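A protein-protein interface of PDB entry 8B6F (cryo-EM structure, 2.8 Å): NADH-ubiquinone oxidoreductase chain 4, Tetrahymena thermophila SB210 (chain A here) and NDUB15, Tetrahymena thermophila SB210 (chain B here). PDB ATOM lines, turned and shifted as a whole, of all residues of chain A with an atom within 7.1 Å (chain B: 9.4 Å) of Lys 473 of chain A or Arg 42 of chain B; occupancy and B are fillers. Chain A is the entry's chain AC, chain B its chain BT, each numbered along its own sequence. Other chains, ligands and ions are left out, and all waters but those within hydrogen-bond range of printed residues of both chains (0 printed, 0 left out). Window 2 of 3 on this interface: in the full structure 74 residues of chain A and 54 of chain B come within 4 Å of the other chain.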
ATOM      1  N   ARG A 384      -4.868 -28.274   2.202  1.00  0.00           N
ATOM      2  CA  ARG A 384      -5.574 -27.918   3.428  1.00  0.00           C
ATOM      3  C   ARG A 384      -6.935 -27.288   3.143  1.00  0.00           C
ATOM      4  O   ARG A 384      -7.928 -27.647   3.784  1.00  0.00           O
ATOM      5  CB  ARG A 384      -4.704 -26.996   4.286  1.00  0.00           C
ATOM      6  CG  ARG A 384      -4.502 -25.600   3.743  1.00  0.00           C
ATOM      7  CD  ARG A 384      -3.444 -24.851   4.542  1.00  0.00           C
ATOM      8  NE  ARG A 384      -2.145 -25.518   4.506  1.00  0.00           N
ATOM      9  CZ  ARG A 384      -1.693 -26.351   5.436  1.00  0.00           C
ATOM     10  NH1 ARG A 384      -2.405 -26.645   6.511  1.00  0.00           N
ATOM     11  NH2 ARG A 384      -0.495 -26.907   5.281  1.00  0.00           N
ATOM     12  N   HIS A 386      -9.614 -27.587   0.366  1.00  0.00           N
ATOM     13  CA  HIS A 386      -9.790 -28.608  -0.659  1.00  0.00           C
ATOM     14  C   HIS A 386     -10.214 -27.980  -1.979  1.00  0.00           C
ATOM     15  O   HIS A 386     -11.229 -28.366  -2.563  1.00  0.00           O
ATOM     16  CB  HIS A 386     -10.807 -29.643  -0.184  1.00  0.00           C
ATOM     17  CG  HIS A 386     -10.506 -30.182   1.179  1.00  0.00           C
ATOM     18  ND1 HIS A 386      -9.526 -31.124   1.404  1.00  0.00           N
ATOM     19  CD2 HIS A 386     -11.038 -29.896   2.389  1.00  0.00           C
ATOM     20  CE1 HIS A 386      -9.474 -31.401   2.694  1.00  0.00           C
ATOM     21  NE2 HIS A 386     -10.380 -30.669   3.314  1.00  0.00           N
ATOM     22  N   LYS A 470     -17.052 -19.017   4.997  1.00  0.00           N
ATOM     23  CA  LYS A 470     -17.676 -20.213   4.450  1.00  0.00           C
ATOM     24  C   LYS A 470     -17.049 -21.472   5.036  1.00  0.00           C
ATOM     25  O   LYS A 470     -15.829 -21.555   5.197  1.00  0.00           O
ATOM     26  CB  LYS A 470     -17.543 -20.224   2.926  1.00  0.00           C
ATOM     27  CG  LYS A 470     -18.265 -21.373   2.246  1.00  0.00           C
ATOM     28  CD  LYS A 470     -18.052 -21.358   0.739  1.00  0.00           C
ATOM     29  CE  LYS A 470     -16.604 -21.645   0.372  1.00  0.00           C
ATOM     30  NZ  LYS A 470     -16.428 -21.808  -1.098  1.00  0.00           N
ATOM     31  N   ASN A 471     -17.895 -22.451   5.349  1.00  0.00           N
ATOM     32  CA  ASN A 471     -17.458 -23.769   5.805  1.00  0.00           C
ATOM     33  C   ASN A 471     -16.504 -23.651   6.993  1.00  0.00           C
ATOM     34  O   ASN A 471     -15.335 -24.034   6.934  1.00  0.00           O
ATOM     35  CB  ASN A 471     -16.806 -24.546   4.659  1.00  0.00           C
ATOM     36  CG  ASN A 471     -17.768 -24.824   3.522  1.00  0.00           C
ATOM     37  OD1 ASN A 471     -18.956 -25.051   3.741  1.00  0.00           O
ATOM     38  ND2 ASN A 471     -17.256 -24.808   2.299  1.00  0.00           N
ATOM     39  N   THR A 472     -17.034 -23.109   8.090  1.00  0.00           N
ATOM     40  CA  THR A 472     -16.219 -22.894   9.279  1.00  0.00           C
ATOM     41  C   THR A 472     -15.880 -24.197   9.994  1.00  0.00           C
ATOM     42  O   THR A 472     -14.918 -24.228  10.767  1.00  0.00           O
ATOM     43  CB  THR A 472     -16.938 -21.941  10.235  1.00  0.00           C
ATOM     44  OG1 THR A 472     -17.176 -20.692   9.576  1.00  0.00           O
ATOM     45  CG2 THR A 472     -16.106 -21.687  11.477  1.00  0.00           C
ATOM     46  N   LYS A 473     -16.631 -25.269   9.749  1.00  0.00           N
ATOM     47  CA  LYS A 473     -16.337 -26.547  10.381  1.00  0.00           C
ATOM     48  C   LYS A 473     -15.161 -27.265   9.740  1.00  0.00           C
ATOM     49  O   LYS A 473     -14.633 -28.208  10.339  1.00  0.00           O
ATOM     50  CB  LYS A 473     -17.562 -27.462  10.319  1.00  0.00           C
ATOM     51  CG  LYS A 473     -18.756 -26.975  11.121  1.00  0.00           C
ATOM     52  CD  LYS A 473     -19.980 -27.855  10.894  1.00  0.00           C
ATOM     53  CE  LYS A 473     -19.736 -29.293  11.330  1.00  0.00           C
ATOM     54  NZ  LYS A 473     -20.951 -30.140  11.165  1.00  0.00           N
ATOM     55  N   TYR A 474     -14.740 -26.846   8.548  1.00  0.00           N
ATOM     56  CA  TYR A 474     -13.744 -27.571   7.770  1.00  0.00           C
ATOM     57  C   TYR A 474     -12.470 -26.766   7.550  1.00  0.00           C
ATOM     58  O   TYR A 474     -11.631 -27.170   6.738  1.00  0.00           O
ATOM     59  CB  TYR A 474     -14.341 -27.981   6.420  1.00  0.00           C
ATOM     60  CG  TYR A 474     -15.700 -28.638   6.532  1.00  0.00           C
ATOM     61  CD1 TYR A 474     -16.854 -27.876   6.664  1.00  0.00           C
ATOM     62  CD2 TYR A 474     -15.828 -30.019   6.501  1.00  0.00           C
ATOM     63  CE1 TYR A 474     -18.094 -28.471   6.765  1.00  0.00           C
ATOM     64  CE2 TYR A 474     -17.063 -30.623   6.601  1.00  0.00           C
ATOM     65  CZ  TYR A 474     -18.193 -29.845   6.733  1.00  0.00           C
ATOM     66  OH  TYR A 474     -19.425 -30.443   6.832  1.00  0.00           O
ATOM     67  N   LEU A 475     -12.299 -25.646   8.244  1.00  0.00           N
ATOM     68  CA  LEU A 475     -11.122 -24.821   8.028  1.00  0.00           C
ATOM     69  C   LEU A 475      -9.873 -25.533   8.545  1.00  0.00           C
ATOM     70  O   LEU A 475      -9.925 -26.203   9.581  1.00  0.00           O
ATOM     71  CB  LEU A 475     -11.277 -23.471   8.721  1.00  0.00           C
ATOM     72  CG  LEU A 475     -12.369 -22.557   8.162  1.00  0.00           C
ATOM     73  CD1 LEU A 475     -12.507 -21.312   9.013  1.00  0.00           C
ATOM     74  CD2 LEU A 475     -12.076 -22.178   6.719  1.00  0.00           C
ATOM     75  N   PRO A 476      -8.742 -25.404   7.861  1.00  0.00           N
ATOM     76  CA  PRO A 476      -7.515 -26.068   8.306  1.00  0.00           C
ATOM     77  C   PRO A 476      -6.863 -25.318   9.464  1.00  0.00           C
ATOM     78  O   PRO A 476      -7.401 -24.344   9.984  1.00  0.00           O
ATOM     79  CB  PRO A 476      -6.644 -26.049   7.052  1.00  0.00           C
ATOM     80  CG  PRO A 476      -7.069 -24.827   6.333  1.00  0.00           C
ATOM     81  CD  PRO A 476      -8.537 -24.661   6.603  1.00  0.00           C
ATOM     82  N   MET A 477      -5.685 -25.799   9.873  1.00  0.00           N
ATOM     83  CA  MET A 477      -4.979 -25.214  11.010  1.00  0.00           C
ATOM     84  C   MET A 477      -3.861 -24.265  10.594  1.00  0.00           C
ATOM     85  O   MET A 477      -3.908 -23.072  10.904  1.00  0.00           O
ATOM     86  CB  MET A 477      -4.375 -26.326  11.874  1.00  0.00           C
ATOM     87  CG  MET A 477      -5.315 -26.941  12.875  1.00  0.00           C
ATOM     88  SD  MET A 477      -4.467 -28.151  13.905  1.00  0.00           S
ATOM     89  CE  MET A 477      -3.237 -27.134  14.722  1.00  0.00           C
ATOM     90  N   ASP B  36      -6.864 -37.541   0.000  1.00  0.00           N
ATOM     91  CA  ASP B  36      -6.029 -36.553   0.667  1.00  0.00           C
ATOM     92  C   ASP B  36      -6.656 -36.244   2.021  1.00  0.00           C
ATOM     93  O   ASP B  36      -7.806 -35.798   2.088  1.00  0.00           O
ATOM     94  CB  ASP B  36      -5.909 -35.291  -0.185  1.00  0.00           C
ATOM     95  CG  ASP B  36      -4.891 -34.317   0.359  1.00  0.00           C
ATOM     96  OD1 ASP B  36      -3.683 -34.626   0.308  1.00  0.00           O
ATOM     97  OD2 ASP B  36      -5.299 -33.237   0.837  1.00  0.00           O
ATOM     98  N   ALA B  37      -5.904 -36.475   3.093  1.00  0.00           N
ATOM     99  CA  ALA B  37      -6.429 -36.444   4.454  1.00  0.00           C
ATOM    100  C   ALA B  37      -5.629 -35.493   5.328  1.00  0.00           C
ATOM    101  O   ALA B  37      -5.252 -35.817   6.456  1.00  0.00           O
ATOM    102  CB  ALA B  37      -6.430 -37.844   5.057  1.00  0.00           C
ATOM    103  N   LEU B  38      -5.356 -34.295   4.821  1.00  0.00           N
ATOM    104  CA  LEU B  38      -4.634 -33.308   5.607  1.00  0.00           C
ATOM    105  C   LEU B  38      -5.591 -32.537   6.503  1.00  0.00           C
ATOM    106  O   LEU B  38      -6.691 -32.162   6.089  1.00  0.00           O
ATOM    107  CB  LEU B  38      -3.890 -32.335   4.694  1.00  0.00           C
ATOM    108  CG  LEU B  38      -2.931 -31.367   5.395  1.00  0.00           C
ATOM    109  CD1 LEU B  38      -1.738 -32.105   5.973  1.00  0.00           C
ATOM    110  CD2 LEU B  38      -2.479 -30.274   4.444  1.00  0.00           C
ATOM    111  N   SER B  39      -5.160 -32.302   7.740  1.00  0.00           N
ATOM    112  CA  SER B  39      -5.912 -31.504   8.705  1.00  0.00           C
ATOM    113  C   SER B  39      -7.250 -32.155   9.057  1.00  0.00           C
ATOM    114  O   SER B  39      -8.299 -31.509   9.062  1.00  0.00           O
ATOM    115  CB  SER B  39      -6.117 -30.082   8.189  1.00  0.00           C
ATOM    116  OG  SER B  39      -6.773 -29.304   9.169  1.00  0.00           O
ATOM    117  N   GLY B  40      -7.206 -33.449   9.358  1.00  0.00           N
ATOM    118  CA  GLY B  40      -8.364 -34.156   9.861  1.00  0.00           C
ATOM    119  C   GLY B  40      -9.275 -34.760   8.814  1.00  0.00           C
ATOM    120  O   GLY B  40     -10.262 -35.408   9.183  1.00  0.00           O
ATOM    121  N   PHE B  41      -8.987 -34.572   7.529  1.00  0.00           N
ATOM    122  CA  PHE B  41      -9.796 -35.145   6.454  1.00  0.00           C
ATOM    123  C   PHE B  41     -11.251 -34.683   6.568  1.00  0.00           C
ATOM    124  O   PHE B  41     -12.182 -35.486   6.667  1.00  0.00           O
ATOM    125  CB  PHE B  41      -9.697 -36.676   6.469  1.00  0.00           C
ATOM    126  CG  PHE B  41     -10.102 -37.338   5.175  1.00  0.00           C
ATOM    127  CD1 PHE B  41     -10.823 -36.655   4.207  1.00  0.00           C
ATOM    128  CD2 PHE B  41      -9.763 -38.657   4.935  1.00  0.00           C
ATOM    129  CE1 PHE B  41     -11.189 -37.274   3.029  1.00  0.00           C
ATOM    130  CE2 PHE B  41     -10.126 -39.281   3.759  1.00  0.00           C
ATOM    131  CZ  PHE B  41     -10.840 -38.589   2.806  1.00  0.00           C
ATOM    132  N   ARG B  42     -11.432 -33.367   6.555  1.00  0.00           N
ATOM    133  CA  ARG B  42     -12.751 -32.749   6.616  1.00  0.00           C
ATOM    134  C   ARG B  42     -13.042 -32.094   5.272  1.00  0.00           C
ATOM    135  O   ARG B  42     -12.315 -31.191   4.850  1.00  0.00           O
ATOM    136  CB  ARG B  42     -12.819 -31.723   7.744  1.00  0.00           C
ATOM    137  CG  ARG B  42     -12.630 -32.314   9.131  1.00  0.00           C
ATOM    138  CD  ARG B  42     -12.466 -31.220  10.168  1.00  0.00           C
ATOM    139  NE  ARG B  42     -11.221 -30.483   9.980  1.00  0.00           N
ATOM    140  CZ  ARG B  42     -10.938 -29.326  10.563  1.00  0.00           C
ATOM    141  NH1 ARG B  42     -11.801 -28.726  11.366  1.00  0.00           N
ATOM    142  NH2 ARG B  42      -9.761 -28.754  10.331  1.00  0.00           N
ATOM    143  N   ILE B  43     -14.108 -32.543   4.615  1.00  0.00           N
ATOM    144  CA  ILE B  43     -14.477 -32.084   3.281  1.00  0.00           C
ATOM    145  C   ILE B  43     -15.842 -31.419   3.373  1.00  0.00           C
ATOM    146  O   ILE B  43     -16.782 -31.999   3.927  1.00  0.00           O
ATOM    147  CB  ILE B  43     -14.506 -33.240   2.265  1.00  0.00           C
ATOM    148  CG1 ILE B  43     -13.269 -34.131   2.413  1.00  0.00           C
ATOM    149  CG2 ILE B  43     -14.612 -32.692   0.849  1.00  0.00           C
ATOM    150  CD1 ILE B  43     -11.966 -33.452   2.081  1.00  0.00           C
ATOM    151  N   ALA B  44     -15.949 -30.211   2.834  1.00  0.00           N
ATOM    152  CA  ALA B  44     -17.207 -29.483   2.810  1.00  0.00           C
ATOM    153  C   ALA B  44     -17.898 -29.664   1.466  1.00  0.00           C
ATOM    154  O   ALA B  44     -17.256 -29.926   0.445  1.00  0.00           O
ATOM    155  CB  ALA B  44     -16.979 -27.994   3.073  1.00  0.00           C
ATOM    156  N   TYR B  45     -19.219 -29.521   1.476  1.00  0.00           N
ATOM    157  CA  TYR B  45     -19.991 -29.616   0.246  1.00  0.00           C
ATOM    158  C   TYR B  45     -19.739 -28.399  -0.635  1.00  0.00           C
ATOM    159  O   TYR B  45     -19.814 -27.257  -0.173  1.00  0.00           O
ATOM    160  CB  TYR B  45     -21.479 -29.743   0.566  1.00  0.00           C
ATOM    161  CG  TYR B  45     -22.304 -30.233  -0.599  1.00  0.00           C
ATOM    162  CD1 TYR B  45     -22.259 -31.563  -0.997  1.00  0.00           C
ATOM    163  CD2 TYR B  45     -23.135 -29.367  -1.298  1.00  0.00           C
ATOM    164  CE1 TYR B  45     -23.013 -32.016  -2.063  1.00  0.00           C
ATOM    165  CE2 TYR B  45     -23.895 -29.810  -2.366  1.00  0.00           C
ATOM    166  CZ  TYR B  45     -23.829 -31.137  -2.742  1.00  0.00           C
ATOM    167  OH  TYR B  45     -24.583 -31.584  -3.802  1.00  0.00           O
ATOM    168  N   ARG B  46     -19.447 -28.646  -1.907  1.00  0.00           N
ATOM    169  CA  ARG B  46     -19.027 -27.591  -2.815  1.00  0.00           C
ATOM    170  C   ARG B  46     -20.236 -26.815  -3.322  1.00  0.00           C
ATOM    171  O   ARG B  46     -21.316 -27.373  -3.531  1.00  0.00           O
ATOM    172  CB  ARG B  46     -18.244 -28.175  -3.991  1.00  0.00           C
ATOM    173  CG  ARG B  46     -17.042 -29.005  -3.572  1.00  0.00           C
ATOM    174  CD  ARG B  46     -16.193 -29.400  -4.766  1.00  0.00           C
ATOM    175  NE  ARG B  46     -15.031 -30.186  -4.369  1.00  0.00           N
ATOM    176  CZ  ARG B  46     -13.913 -29.679  -3.871  1.00  0.00           C
ATOM    177  NH1 ARG B  46     -13.769 -28.378  -3.678  1.00  0.00           N
ATOM    178  NH2 ARG B  46     -12.913 -30.497  -3.557  1.00  0.00           N
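Among the printed residues, pairs that only touch across the chains: Arg 384 of chain A with Leu 38 of chain B, His 386 of chain A with Ile 43 of chain B, Asn 471 of chain A with Ala 44 of chain B, Tyr 474 of chain A with Arg 42 of chain B, Tyr 474 of chain A with Ile 43 of chain B, Tyr 474 of chain A with Ala 44 of chain B, Pro 476 of chain A with Ser 39 of chain B and Met 477 of chain A with Ser 39 of chain B.
NE of Arg 42 of chain B sits at hydrogen-bond distance from O of Ser 39 of chain B (3.2 Å).
The backbone carbonyl oxygen (O) of Lys 473 of chain A is in hydrogen-bond range of the guanidinium group (NH1) of Arg 42 of chain B, at 3.1 Å.
O of His 386 of chain A sits at hydrogen-bond distance from NH1 of Arg 46 of chain B (2.8 Å).
The backbone carbonyl oxygen (O) of Leu 475 of chain A is in hydrogen-bond range of the guanidinium group (NH2) of Arg 42 of chain B, at 2.7 Å.
A ring nitrogen (NE2) of His 386 of chain A is in hydrogen-bond range of the backbone carbonyl oxygen of Arg 42 of chain B (2.5 Å).
Of chain B, only Arg 42 (3.1 Å) comes within 4 Å of Lys 473 of chain A.
Of chain B, only Arg 42, Ile 43 and Ala 44 come within 4 Å of Tyr 474 of chain A.
Of the printed residues of chain A, Arg 46 of chain B touches His 386 (2.8 Å).
Of the printed residues of chain B, Pro 476 of chain A touches Ser 39 (3.4 Å).
Printed residues of chain A within 4 Å of Leu 38 of chain B: Arg 384 (3.8 Å).
Of the printed residues of chain A, Ala 44 of chain B touches Asn 471 (3.3 Å) and Tyr 474 (3.6 Å).
Of the printed residues of chain A, Ser 39 of chain B touches Pro 476 and Met 477.
Phe 41 of chain B touches none of the printed residues of chain A.
The nearest residue of chain B that does not touch Lys 473 of chain A is Ala 44 of chain B (6.9 Å).
The nearest residue of chain A that does not touch Arg 42 of chain B is Pro 476 of chain A (4.04 Å).
The nearest printed residue of chain B that does not touch Met 477 of chain A is Arg 42 of chain B (5.1 Å).
Of the 10 printed residues of chain A, 8 touch a printed residue of chain B.
Printed residues of chain A that touch a printed residue of chain B: Arg 384, His 386, Asn 471, Lys 473, Tyr 474, Leu 475, Pro 476 and Met 477.
Hydrophobic or aromatic side chains of chain A within 4 Å of the printed part of chain B: His 386, Tyr 474 and Pro 476.
Among the printed residues, no Asp or Glu carboxylate lies within 4 Å of a Lys or Arg side-chain nitrogen of the other chain.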
